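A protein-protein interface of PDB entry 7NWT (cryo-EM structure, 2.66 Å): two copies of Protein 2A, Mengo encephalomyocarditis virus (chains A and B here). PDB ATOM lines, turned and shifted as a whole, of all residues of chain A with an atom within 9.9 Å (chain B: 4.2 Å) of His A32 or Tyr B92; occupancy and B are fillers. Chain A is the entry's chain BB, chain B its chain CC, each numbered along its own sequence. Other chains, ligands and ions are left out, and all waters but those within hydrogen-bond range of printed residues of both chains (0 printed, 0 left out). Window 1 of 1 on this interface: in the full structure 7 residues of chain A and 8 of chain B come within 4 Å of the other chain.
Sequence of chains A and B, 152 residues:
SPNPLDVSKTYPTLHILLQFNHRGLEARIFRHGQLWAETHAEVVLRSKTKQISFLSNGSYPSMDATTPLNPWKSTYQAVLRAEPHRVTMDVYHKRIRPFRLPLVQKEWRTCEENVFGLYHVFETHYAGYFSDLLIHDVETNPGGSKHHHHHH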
ATOM      1  N   SER A   8     -20.148   6.030 -36.332  1.00  0.00           N
ATOM      2  CA  SER A   8     -19.544   4.889 -35.666  1.00  0.00           C
ATOM      3  C   SER A   8     -18.670   4.094 -36.627  1.00  0.00           C
ATOM      4  O   SER A   8     -18.934   4.025 -37.830  1.00  0.00           O
ATOM      5  CB  SER A   8     -20.618   3.982 -35.070  1.00  0.00           C
ATOM      6  OG  SER A   8     -21.380   4.674 -34.098  1.00  0.00           O
ATOM      7  N   THR A  10     -17.765   0.715 -35.839  1.00  0.00           N
ATOM      8  CA  THR A  10     -17.827  -0.560 -35.143  1.00  0.00           C
ATOM      9  C   THR A  10     -18.002  -1.685 -36.152  1.00  0.00           C
ATOM     10  O   THR A  10     -19.037  -1.778 -36.818  1.00  0.00           O
ATOM     11  CB  THR A  10     -18.969  -0.552 -34.135  1.00  0.00           C
ATOM     12  OG1 THR A  10     -20.209  -0.396 -34.833  1.00  0.00           O
ATOM     13  CG2 THR A  10     -18.787   0.604 -33.168  1.00  0.00           C
ATOM     14  N   TYR A  11     -17.002  -2.547 -36.233  1.00  0.00           N
ATOM     15  CA  TYR A  11     -16.910  -3.642 -37.184  1.00  0.00           C
ATOM     16  C   TYR A  11     -16.514  -4.869 -36.382  1.00  0.00           C
ATOM     17  O   TYR A  11     -16.369  -4.764 -35.160  1.00  0.00           O
ATOM     18  CB  TYR A  11     -15.875  -3.329 -38.264  1.00  0.00           C
ATOM     19  CG  TYR A  11     -16.034  -1.974 -38.899  1.00  0.00           C
ATOM     20  CD1 TYR A  11     -17.264  -1.545 -39.359  1.00  0.00           C
ATOM     21  CD2 TYR A  11     -14.950  -1.122 -39.032  1.00  0.00           C
ATOM     22  CE1 TYR A  11     -17.413  -0.307 -39.938  1.00  0.00           C
ATOM     23  CE2 TYR A  11     -15.089   0.119 -39.610  1.00  0.00           C
ATOM     24  CZ  TYR A  11     -16.323   0.521 -40.062  1.00  0.00           C
ATOM     25  OH  TYR A  11     -16.471   1.758 -40.641  1.00  0.00           O
ATOM     26  N   PRO A  12     -16.345  -6.040 -36.991  1.00  0.00           N
ATOM     27  CA  PRO A  12     -15.680  -7.121 -36.265  1.00  0.00           C
ATOM     28  C   PRO A  12     -14.313  -6.661 -35.786  1.00  0.00           C
ATOM     29  O   PRO A  12     -13.569  -5.999 -36.510  1.00  0.00           O
ATOM     30  CB  PRO A  12     -15.579  -8.232 -37.310  1.00  0.00           C
ATOM     31  CG  PRO A  12     -16.771  -8.010 -38.150  1.00  0.00           C
ATOM     32  CD  PRO A  12     -16.894  -6.519 -38.271  1.00  0.00           C
ATOM     33  N   THR A  13     -13.990  -7.019 -34.549  1.00  0.00           N
ATOM     34  CA  THR A  13     -12.719  -6.657 -33.946  1.00  0.00           C
ATOM     35  C   THR A  13     -12.169  -7.836 -33.167  1.00  0.00           C
ATOM     36  O   THR A  13     -12.919  -8.560 -32.510  1.00  0.00           O
ATOM     37  CB  THR A  13     -12.861  -5.436 -33.033  1.00  0.00           C
ATOM     38  OG1 THR A  13     -13.312  -4.317 -33.802  1.00  0.00           O
ATOM     39  CG2 THR A  13     -11.535  -5.082 -32.407  1.00  0.00           C
ATOM     40  N   LEU A  14     -10.860  -8.021 -33.242  1.00  0.00           N
ATOM     41  CA  LEU A  14     -10.158  -8.968 -32.397  1.00  0.00           C
ATOM     42  C   LEU A  14      -9.008  -8.264 -31.705  1.00  0.00           C
ATOM     43  O   LEU A  14      -8.286  -7.476 -32.319  1.00  0.00           O
ATOM     44  CB  LEU A  14      -9.629 -10.153 -33.188  1.00  0.00           C
ATOM     45  CG  LEU A  14     -10.702 -11.073 -33.744  1.00  0.00           C
ATOM     46  CD1 LEU A  14     -10.070 -12.134 -34.609  1.00  0.00           C
ATOM     47  CD2 LEU A  14     -11.445 -11.702 -32.591  1.00  0.00           C
ATOM     48  N   HIS A  15      -8.865  -8.539 -30.416  1.00  0.00           N
ATOM     49  CA  HIS A  15      -7.709  -8.133 -29.636  1.00  0.00           C
ATOM     50  C   HIS A  15      -6.889  -9.379 -29.343  1.00  0.00           C
ATOM     51  O   HIS A  15      -7.407 -10.348 -28.785  1.00  0.00           O
ATOM     52  CB  HIS A  15      -8.173  -7.450 -28.355  1.00  0.00           C
ATOM     53  CG  HIS A  15      -7.066  -7.023 -27.448  1.00  0.00           C
ATOM     54  ND1 HIS A  15      -7.289  -6.643 -26.143  1.00  0.00           N
ATOM     55  CD2 HIS A  15      -5.733  -6.916 -27.649  1.00  0.00           C
ATOM     56  CE1 HIS A  15      -6.141  -6.321 -25.580  1.00  0.00           C
ATOM     57  NE2 HIS A  15      -5.180  -6.478 -26.471  1.00  0.00           N
ATOM     58  N   ILE A  16      -5.618  -9.355 -29.723  1.00  0.00           N
ATOM     59  CA  ILE A  16      -4.734 -10.506 -29.598  1.00  0.00           C
ATOM     60  C   ILE A  16      -3.555 -10.127 -28.730  1.00  0.00           C
ATOM     61  O   ILE A  16      -2.714  -9.318 -29.136  1.00  0.00           O
ATOM     62  CB  ILE A  16      -4.245 -11.029 -30.951  1.00  0.00           C
ATOM     63  CG1 ILE A  16      -5.412 -11.299 -31.881  1.00  0.00           C
ATOM     64  CG2 ILE A  16      -3.407 -12.276 -30.761  1.00  0.00           C
ATOM     65  CD1 ILE A  16      -4.996 -12.016 -33.111  1.00  0.00           C
ATOM     66  N   ILE A  29      -6.382 -14.739 -27.824  1.00  0.00           N
ATOM     67  CA  ILE A  29      -7.359 -13.958 -28.578  1.00  0.00           C
ATOM     68  C   ILE A  29      -8.535 -13.596 -27.687  1.00  0.00           C
ATOM     69  O   ILE A  29      -9.190 -14.479 -27.124  1.00  0.00           O
ATOM     70  CB  ILE A  29      -7.830 -14.713 -29.825  1.00  0.00           C
ATOM     71  CG1 ILE A  29      -6.621 -15.289 -30.550  1.00  0.00           C
ATOM     72  CG2 ILE A  29      -8.598 -13.783 -30.725  1.00  0.00           C
ATOM     73  CD1 ILE A  29      -6.963 -16.032 -31.802  1.00  0.00           C
ATOM     74  N   PHE A  30      -8.823 -12.306 -27.575  1.00  0.00           N
ATOM     75  CA  PHE A  30      -9.921 -11.821 -26.756  1.00  0.00           C
ATOM     76  C   PHE A  30     -11.026 -11.244 -27.624  1.00  0.00           C
ATOM     77  O   PHE A  30     -10.779 -10.683 -28.694  1.00  0.00           O
ATOM     78  CB  PHE A  30      -9.448 -10.764 -25.764  1.00  0.00           C
ATOM     79  CG  PHE A  30      -8.602 -11.315 -24.681  1.00  0.00           C
ATOM     80  CD1 PHE A  30      -7.253 -11.507 -24.876  1.00  0.00           C
ATOM     81  CD2 PHE A  30      -9.159 -11.665 -23.472  1.00  0.00           C
ATOM     82  CE1 PHE A  30      -6.475 -12.029 -23.883  1.00  0.00           C
ATOM     83  CE2 PHE A  30      -8.386 -12.187 -22.474  1.00  0.00           C
ATOM     84  CZ  PHE A  30      -7.040 -12.370 -22.678  1.00  0.00           C
ATOM     85  N   ARG A  31     -12.253 -11.385 -27.137  1.00  0.00           N
ATOM     86  CA  ARG A  31     -13.453 -11.032 -27.885  1.00  0.00           C
ATOM     87  C   ARG A  31     -14.440 -10.440 -26.893  1.00  0.00           C
ATOM     88  O   ARG A  31     -14.936 -11.150 -26.015  1.00  0.00           O
ATOM     89  CB  ARG A  31     -14.031 -12.246 -28.600  1.00  0.00           C
ATOM     90  CG  ARG A  31     -15.248 -11.949 -29.420  1.00  0.00           C
ATOM     91  CD  ARG A  31     -15.676 -13.194 -30.152  1.00  0.00           C
ATOM     92  NE  ARG A  31     -16.959 -13.021 -30.818  1.00  0.00           N
ATOM     93  CZ  ARG A  31     -17.646 -14.008 -31.371  1.00  0.00           C
ATOM     94  NH1 ARG A  31     -17.210 -15.256 -31.336  1.00  0.00           N
ATOM     95  NH2 ARG A  31     -18.805 -13.739 -31.963  1.00  0.00           N
ATOM     96  N   HIS A  32     -14.708  -9.142 -27.026  1.00  0.00           N
ATOM     97  CA  HIS A  32     -15.488  -8.388 -26.046  1.00  0.00           C
ATOM     98  C   HIS A  32     -14.881  -8.554 -24.660  1.00  0.00           C
ATOM     99  O   HIS A  32     -15.584  -8.635 -23.655  1.00  0.00           O
ATOM    100  CB  HIS A  32     -16.953  -8.835 -26.024  1.00  0.00           C
ATOM    101  CG  HIS A  32     -17.623  -8.812 -27.360  1.00  0.00           C
ATOM    102  ND1 HIS A  32     -17.835  -9.953 -28.101  1.00  0.00           N
ATOM    103  CD2 HIS A  32     -18.137  -7.791 -28.085  1.00  0.00           C
ATOM    104  CE1 HIS A  32     -18.445  -9.637 -29.228  1.00  0.00           C
ATOM    105  NE2 HIS A  32     -18.639  -8.331 -29.244  1.00  0.00           N
ATOM    106  N   GLY A  33     -13.554  -8.598 -24.610  1.00  0.00           N
ATOM    107  CA  GLY A  33     -12.870  -8.782 -23.350  1.00  0.00           C
ATOM    108  C   GLY A  33     -12.938 -10.187 -22.807  1.00  0.00           C
ATOM    109  O   GLY A  33     -12.494 -10.425 -21.683  1.00  0.00           O
ATOM    110  N   GLN A  34     -13.464 -11.130 -23.577  1.00  0.00           N
ATOM    111  CA  GLN A  34     -13.553 -12.522 -23.167  1.00  0.00           C
ATOM    112  C   GLN A  34     -12.510 -13.342 -23.905  1.00  0.00           C
ATOM    113  O   GLN A  34     -12.431 -13.286 -25.136  1.00  0.00           O
ATOM    114  CB  GLN A  34     -14.948 -13.071 -23.450  1.00  0.00           C
ATOM    115  CG  GLN A  34     -16.054 -12.197 -22.896  1.00  0.00           C
ATOM    116  CD  GLN A  34     -15.931 -11.963 -21.413  1.00  0.00           C
ATOM    117  OE1 GLN A  34     -15.845 -10.824 -20.962  1.00  0.00           O
ATOM    118  NE2 GLN A  34     -15.921 -13.041 -20.641  1.00  0.00           N
ATOM    119  N   LEU A  35     -11.706 -14.092 -23.156  1.00  0.00           N
ATOM    120  CA  LEU A  35     -10.724 -14.963 -23.781  1.00  0.00           C
ATOM    121  C   LEU A  35     -11.479 -15.964 -24.636  1.00  0.00           C
ATOM    122  O   LEU A  35     -12.168 -16.846 -24.117  1.00  0.00           O
ATOM    123  CB  LEU A  35      -9.860 -15.657 -22.728  1.00  0.00           C
ATOM    124  CG  LEU A  35      -8.758 -16.618 -23.182  1.00  0.00           C
ATOM    125  CD1 LEU A  35      -9.270 -18.041 -23.326  1.00  0.00           C
ATOM    126  CD2 LEU A  35      -8.121 -16.148 -24.480  1.00  0.00           C
ATOM    127  N   TRP A  36     -11.369 -15.821 -25.949  1.00  0.00           N
ATOM    128  CA  TRP A  36     -12.110 -16.658 -26.873  1.00  0.00           C
ATOM    129  C   TRP A  36     -11.312 -17.856 -27.377  1.00  0.00           C
ATOM    130  O   TRP A  36     -11.876 -18.942 -27.522  1.00  0.00           O
ATOM    131  CB  TRP A  36     -12.595 -15.805 -28.045  1.00  0.00           C
ATOM    132  CG  TRP A  36     -13.229 -16.564 -29.130  1.00  0.00           C
ATOM    133  CD1 TRP A  36     -14.288 -17.409 -29.015  1.00  0.00           C
ATOM    134  CD2 TRP A  36     -12.883 -16.536 -30.512  1.00  0.00           C
ATOM    135  NE1 TRP A  36     -14.619 -17.920 -30.241  1.00  0.00           N
ATOM    136  CE2 TRP A  36     -13.768 -17.400 -31.179  1.00  0.00           C
ATOM    137  CE3 TRP A  36     -11.907 -15.872 -31.251  1.00  0.00           C
ATOM    138  CZ2 TRP A  36     -13.705 -17.617 -32.547  1.00  0.00           C
ATOM    139  CZ3 TRP A  36     -11.846 -16.088 -32.608  1.00  0.00           C
ATOM    140  CH2 TRP A  36     -12.738 -16.953 -33.243  1.00  0.00           C
ATOM    141  N   ALA A  37     -10.016 -17.699 -27.642  1.00  0.00           N
ATOM    142  CA  ALA A  37      -9.230 -18.776 -28.230  1.00  0.00           C
ATOM    143  C   ALA A  37      -7.773 -18.659 -27.799  1.00  0.00           C
ATOM    144  O   ALA A  37      -7.315 -17.602 -27.362  1.00  0.00           O
ATOM    145  CB  ALA A  37      -9.339 -18.773 -29.755  1.00  0.00           C
ATOM    146  N   VAL A 115     -15.564 -12.847 -37.553  1.00  0.00           N
ATOM    147  CA  VAL A 115     -14.328 -12.996 -36.791  1.00  0.00           C
ATOM    148  C   VAL A 115     -13.502 -14.174 -37.286  1.00  0.00           C
ATOM    149  O   VAL A 115     -12.267 -14.133 -37.246  1.00  0.00           O
ATOM    150  CB  VAL A 115     -14.636 -13.120 -35.290  1.00  0.00           C
ATOM    151  CG1 VAL A 115     -15.183 -11.811 -34.762  1.00  0.00           C
ATOM    152  CG2 VAL A 115     -15.612 -14.248 -35.043  1.00  0.00           C
ATOM    153  N   TYR B  76     -30.468   3.113 -26.733  1.00  0.00           N
ATOM    154  CA  TYR B  76     -29.641   1.927 -26.872  1.00  0.00           C
ATOM    155  C   TYR B  76     -29.318   1.739 -28.345  1.00  0.00           C
ATOM    156  O   TYR B  76     -30.006   2.268 -29.220  1.00  0.00           O
ATOM    157  CB  TYR B  76     -30.352   0.679 -26.345  1.00  0.00           C
ATOM    158  CG  TYR B  76     -30.772   0.760 -24.902  1.00  0.00           C
ATOM    159  CD1 TYR B  76     -31.986   1.321 -24.548  1.00  0.00           C
ATOM    160  CD2 TYR B  76     -29.973   0.244 -23.898  1.00  0.00           C
ATOM    161  CE1 TYR B  76     -32.379   1.393 -23.233  1.00  0.00           C
ATOM    162  CE2 TYR B  76     -30.361   0.310 -22.577  1.00  0.00           C
ATOM    163  CZ  TYR B  76     -31.565   0.885 -22.249  1.00  0.00           C
ATOM    164  OH  TYR B  76     -31.964   0.951 -20.934  1.00  0.00           O
ATOM    165  N   GLN B  77     -28.261   0.977 -28.617  1.00  0.00           N
ATOM    166  CA  GLN B  77     -27.925   0.575 -29.977  1.00  0.00           C
ATOM    167  C   GLN B  77     -27.819  -0.937 -30.047  1.00  0.00           C
ATOM    168  O   GLN B  77     -26.982  -1.533 -29.367  1.00  0.00           O
ATOM    169  CB  GLN B  77     -26.609   1.198 -30.440  1.00  0.00           C
ATOM    170  CG  GLN B  77     -26.550   2.697 -30.371  1.00  0.00           C
ATOM    171  CD  GLN B  77     -26.139   3.206 -29.015  1.00  0.00           C
ATOM    172  OE1 GLN B  77     -26.125   2.463 -28.035  1.00  0.00           O
ATOM    173  NE2 GLN B  77     -25.790   4.484 -28.950  1.00  0.00           N
ATOM    174  N   VAL B  79     -26.690  -3.953 -32.516  1.00  0.00           N
ATOM    175  CA  VAL B  79     -25.900  -4.273 -33.699  1.00  0.00           C
ATOM    176  C   VAL B  79     -26.142  -5.735 -34.055  1.00  0.00           C
ATOM    177  O   VAL B  79     -25.866  -6.630 -33.248  1.00  0.00           O
ATOM    178  CB  VAL B  79     -24.404  -3.986 -33.491  1.00  0.00           C
ATOM    179  CG1 VAL B  79     -23.939  -4.476 -32.133  1.00  0.00           C
ATOM    180  CG2 VAL B  79     -23.588  -4.621 -34.598  1.00  0.00           C
ATOM    181  N   ASP B  90     -26.202  -7.531 -30.218  1.00  0.00           N
ATOM    182  CA  ASP B  90     -25.735  -6.953 -28.966  1.00  0.00           C
ATOM    183  C   ASP B  90     -26.234  -5.521 -28.866  1.00  0.00           C
ATOM    184  O   ASP B  90     -26.080  -4.735 -29.805  1.00  0.00           O
ATOM    185  CB  ASP B  90     -24.213  -6.985 -28.860  1.00  0.00           C
ATOM    186  CG  ASP B  90     -23.658  -8.383 -28.921  1.00  0.00           C
ATOM    187  OD1 ASP B  90     -24.458  -9.332 -29.044  1.00  0.00           O
ATOM    188  OD2 ASP B  90     -22.425  -8.538 -28.820  1.00  0.00           O
ATOM    189  N   VAL B  91     -26.838  -5.197 -27.730  1.00  0.00           N
ATOM    190  CA  VAL B  91     -27.434  -3.893 -27.473  1.00  0.00           C
ATOM    191  C   VAL B  91     -26.666  -3.211 -26.352  1.00  0.00           C
ATOM    192  O   VAL B  91     -26.476  -3.803 -25.283  1.00  0.00           O
ATOM    193  CB  VAL B  91     -28.923  -4.016 -27.124  1.00  0.00           C
ATOM    194  CG1 VAL B  91     -29.583  -2.660 -27.126  1.00  0.00           C
ATOM    195  CG2 VAL B  91     -29.610  -4.964 -28.084  1.00  0.00           C
ATOM    196  N   TYR B  92     -26.218  -1.982 -26.586  1.00  0.00           N
ATOM    197  CA  TYR B  92     -25.407  -1.292 -25.598  1.00  0.00           C
ATOM    198  C   TYR B  92     -26.196  -0.113 -25.050  1.00  0.00           C
ATOM    199  O   TYR B  92     -26.859   0.607 -25.800  1.00  0.00           O
ATOM    200  CB  TYR B  92     -24.113  -0.773 -26.227  1.00  0.00           C
ATOM    201  CG  TYR B  92     -23.172  -1.846 -26.705  1.00  0.00           C
ATOM    202  CD1 TYR B  92     -23.304  -2.390 -27.971  1.00  0.00           C
ATOM    203  CD2 TYR B  92     -22.148  -2.310 -25.899  1.00  0.00           C
ATOM    204  CE1 TYR B  92     -22.452  -3.372 -28.418  1.00  0.00           C
ATOM    205  CE2 TYR B  92     -21.289  -3.291 -26.338  1.00  0.00           C
ATOM    206  CZ  TYR B  92     -21.444  -3.819 -27.598  1.00  0.00           C
ATOM    207  OH  TYR B  92     -20.588  -4.794 -28.042  1.00  0.00           O
ATOM    208  N   HIS B  93     -26.092   0.092 -23.744  1.00  0.00           N
ATOM    209  CA  HIS B  93     -26.565   1.312 -23.107  1.00  0.00           C
ATOM    210  C   HIS B  93     -25.745   2.517 -23.545  1.00  0.00           C
ATOM    211  O   HIS B  93     -24.512   2.482 -23.495  1.00  0.00           O
ATOM    212  CB  HIS B  93     -26.532   1.173 -21.591  1.00  0.00           C
ATOM    213  CG  HIS B  93     -26.962   2.410 -20.871  1.00  0.00           C
ATOM    214  ND1 HIS B  93     -28.203   2.980 -21.057  1.00  0.00           N
ATOM    215  CD2 HIS B  93     -26.321   3.188 -19.968  1.00  0.00           C
ATOM    216  CE1 HIS B  93     -28.310   4.053 -20.295  1.00  0.00           C
ATOM    217  NE2 HIS B  93     -27.182   4.202 -19.625  1.00  0.00           N
ATOM    218  N   LYS B  94     -26.422   3.564 -24.017  1.00  0.00           N
ATOM    219  CA  LYS B  94     -25.742   4.764 -24.498  1.00  0.00           C
ATOM    220  C   LYS B  94     -24.962   4.530 -25.783  1.00  0.00           C
ATOM    221  O   LYS B  94     -25.347   5.072 -26.822  1.00  0.00           O
ATOM    222  CB  LYS B  94     -24.848   5.359 -23.410  1.00  0.00           C
ATOM    223  CG  LYS B  94     -25.649   6.022 -22.312  1.00  0.00           C
ATOM    224  CD  LYS B  94     -24.797   6.381 -21.120  1.00  0.00           C
ATOM    225  CE  LYS B  94     -25.627   7.137 -20.098  1.00  0.00           C
ATOM    226  NZ  LYS B  94     -26.317   8.294 -20.719  1.00  0.00           N
ATOM    227  N   ARG B  95     -23.897   3.725 -25.764  1.00  0.00           N
ATOM    228  CA  ARG B  95     -23.101   3.588 -26.979  1.00  0.00           C
ATOM    229  C   ARG B  95     -22.342   2.271 -27.004  1.00  0.00           C
ATOM    230  O   ARG B  95     -22.051   1.658 -25.975  1.00  0.00           O
ATOM    231  CB  ARG B  95     -22.061   4.711 -27.133  1.00  0.00           C
ATOM    232  CG  ARG B  95     -22.550   6.144 -27.092  1.00  0.00           C
ATOM    233  CD  ARG B  95     -21.483   7.061 -26.546  1.00  0.00           C
ATOM    234  NE  ARG B  95     -21.896   8.456 -26.599  1.00  0.00           N
ATOM    235  CZ  ARG B  95     -21.512   9.310 -27.535  1.00  0.00           C
ATOM    236  NH1 ARG B  95     -20.699   8.943 -28.511  1.00  0.00           N
ATOM    237  NH2 ARG B  95     -21.948  10.565 -27.486  1.00  0.00           N
ATOM    238  N   ILE B  96     -22.005   1.886 -28.233  1.00  0.00           N
ATOM    239  CA  ILE B  96     -21.226   0.702 -28.581  1.00  0.00           C
ATOM    240  C   ILE B  96     -19.782   0.818 -28.118  1.00  0.00           C
ATOM    241  O   ILE B  96     -19.066   1.754 -28.488  1.00  0.00           O
ATOM    242  CB  ILE B  96     -21.284   0.437 -30.088  1.00  0.00           C
ATOM    243  CG1 ILE B  96     -22.726   0.504 -30.586  1.00  0.00           C
ATOM    244  CG2 ILE B  96     -20.662  -0.908 -30.403  1.00  0.00           C
ATOM    245  CD1 ILE B  96     -23.072   1.792 -31.290  1.00  0.00           C
ATOM    246  N   ARG B  97     -19.359  -0.125 -27.287  1.00  0.00           N
ATOM    247  CA  ARG B  97     -17.982  -0.198 -26.812  1.00  0.00           C
ATOM    248  C   ARG B  97     -17.574  -1.648 -27.016  1.00  0.00           C
ATOM    249  O   ARG B  97     -18.118  -2.544 -26.338  1.00  0.00           O
ATOM    250  CB  ARG B  97     -17.858   0.244 -25.358  1.00  0.00           C
ATOM    251  CG  ARG B  97     -18.070   1.735 -25.232  1.00  0.00           C
ATOM    252  CD  ARG B  97     -17.675   2.301 -23.895  1.00  0.00           C
ATOM    253  NE  ARG B  97     -17.628   3.754 -23.985  1.00  0.00           N
ATOM    254  CZ  ARG B  97     -17.395   4.569 -22.967  1.00  0.00           C
ATOM    255  NH1 ARG B  97     -17.184   4.106 -21.747  1.00  0.00           N
ATOM    256  NH2 ARG B  97     -17.371   5.881 -23.181  1.00  0.00           N
ATOM    257  N   PRO B  98     -16.629  -1.928 -27.914  1.00  0.00           N
ATOM    258  CA  PRO B  98     -16.348  -3.323 -28.274  1.00  0.00           C
ATOM    259  C   PRO B  98     -15.367  -4.024 -27.355  1.00  0.00           C
ATOM    260  O   PRO B  98     -15.356  -5.256 -27.282  1.00  0.00           O
ATOM    261  CB  PRO B  98     -15.761  -3.194 -29.684  1.00  0.00           C
ATOM    262  CG  PRO B  98     -15.143  -1.843 -29.688  1.00  0.00           C
ATOM    263  CD  PRO B  98     -16.054  -0.982 -28.882  1.00  0.00           C
ATOM    264  N   PHE B  99     -14.528  -3.264 -26.662  1.00  0.00           N
ATOM    265  CA  PHE B  99     -13.621  -3.877 -25.707  1.00  0.00           C
ATOM    266  C   PHE B  99     -14.311  -4.167 -24.384  1.00  0.00           C
ATOM    267  O   PHE B  99     -13.834  -5.013 -23.621  1.00  0.00           O
ATOM    268  CB  PHE B  99     -12.393  -2.997 -25.521  1.00  0.00           C
ATOM    269  CG  PHE B  99     -11.537  -2.909 -26.750  1.00  0.00           C
ATOM    270  CD1 PHE B  99     -11.814  -1.981 -27.732  1.00  0.00           C
ATOM    271  CD2 PHE B  99     -10.466  -3.764 -26.927  1.00  0.00           C
ATOM    272  CE1 PHE B  99     -11.036  -1.904 -28.865  1.00  0.00           C
ATOM    273  CE2 PHE B  99      -9.683  -3.689 -28.058  1.00  0.00           C
ATOM    274  CZ  PHE B  99      -9.969  -2.761 -29.027  1.00  0.00           C
ATOM    275  N   ARG B 100     -15.416  -3.485 -24.103  1.00  0.00           N
ATOM    276  CA  ARG B 100     -16.230  -3.757 -22.932  1.00  0.00           C
ATOM    277  C   ARG B 100     -17.261  -4.818 -23.283  1.00  0.00           C
ATOM    278  O   ARG B 100     -17.479  -5.148 -24.449  1.00  0.00           O
ATOM    279  CB  ARG B 100     -16.931  -2.493 -22.442  1.00  0.00           C
ATOM    280  CG  ARG B 100     -16.035  -1.293 -22.280  1.00  0.00           C
ATOM    281  CD  ARG B 100     -14.967  -1.527 -21.243  1.00  0.00           C
ATOM    282  NE  ARG B 100     -14.117  -0.352 -21.103  1.00  0.00           N
ATOM    283  CZ  ARG B 100     -13.002  -0.153 -21.788  1.00  0.00           C
ATOM    284  NH1 ARG B 100     -12.565  -1.036 -22.670  1.00  0.00           N
ATOM    285  NH2 ARG B 100     -12.304   0.961 -21.582  1.00  0.00           N
ATOM    286  N   LEU B 101     -17.889  -5.356 -22.277  1.00  0.00           N
ATOM    287  CA  LEU B 101     -18.754  -6.468 -22.618  1.00  0.00           C
ATOM    288  C   LEU B 101     -20.159  -5.971 -22.932  1.00  0.00           C
ATOM    289  O   LEU B 101     -20.572  -4.909 -22.461  1.00  0.00           O
ATOM    290  CB  LEU B 101     -18.777  -7.451 -21.445  1.00  0.00           C
ATOM    291  CG  LEU B 101     -19.744  -8.623 -21.295  1.00  0.00           C
ATOM    292  CD1 LEU B 101     -19.099  -9.902 -21.786  1.00  0.00           C
ATOM    293  CD2 LEU B 101     -20.184  -8.765 -19.859  1.00  0.00           C
ATOM    294  N   PRO B 102     -20.920  -6.709 -23.741  1.00  0.00           N
ATOM    295  CA  PRO B 102     -22.292  -6.288 -24.042  1.00  0.00           C
ATOM    296  C   PRO B 102     -23.144  -6.326 -22.785  1.00  0.00           C
ATOM    297  O   PRO B 102     -22.960  -7.181 -21.918  1.00  0.00           O
ATOM    298  CB  PRO B 102     -22.753  -7.292 -25.100  1.00  0.00           C
ATOM    299  CG  PRO B 102     -21.898  -8.477 -24.896  1.00  0.00           C
ATOM    300  CD  PRO B 102     -20.566  -7.944 -24.462  1.00  0.00           C
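The backbone carbonyl oxygen (O) of His A32 lies close to the side-chain amide oxygen (OE1) of Gln A34 (3.5 Å).
N of Val B79 lies within hydrogen-bond range of O of Asp B90.
The backbone carbonyl oxygen of Gln B77 sits at hydrogen-bond distance from the backbone NH of Tyr B92 (2.9 Å).
Ile B96 touches Thr A10 (CG2 to CG2, 3.7 Å).
His A32 touches Asp B90.
OH of Tyr B92 touches CD2 of His A32, at 3.9 Å.
CA of His A32 touches O of Pro B98 (3.4 Å).
O of Phe B99 touches C of His A32 (3.8 Å).
CA of Leu B101 touches O of His A32, at 3.98 Å.
Gly A33 touches Phe B99 (N to O, 3.7 Å).
Leu B101 touches Gln A34 (CD1 to OE1, 3.5 Å).
His A32 touches just these residues of chain B: Asp B90, Tyr B92, Pro B98, Phe B99 and Leu B101.
Tyr B92 touches one residue of chain A.
No residue of chain A comes within 4 Å of Val B91.
Ile B96 touches just one residue of chain A: Thr A10 (3.7 Å).
Of the printed residues of chain B, Thr A10 touches Ile B96 (3.7 Å).
Of the printed residues of chain A, Phe B99 touches His A32 (3.8 Å) and Gly A33 (3.7 Å).
Of the printed residues of chain A, Asp B90 touches His A32 (3.8 Å).
Arg A31 touches none of the printed residues of chain B.
His B93 touches none of the printed residues of chain A.
Hydrophobic or aromatic side chains of chain B that line the printed part of chain A: Tyr B92, Ile B96 and Leu B101.
Printed residues of chain A that touch a printed residue of chain B: Thr A10, His A32, Gly A33 and Gln A34.
Hydrophobic or aromatic side chains of chain A within 4 Å of the printed part of chain B: His A32.
Among the printed residues, no Asp or Glu carboxylate lies within 4 Å of a Lys or Arg side-chain nitrogen of the other chain.
No position is printed for both chains.
Of the 8 pairs that touch across the chains among the printed residues, none has its exchanged pair printed and touching as well.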
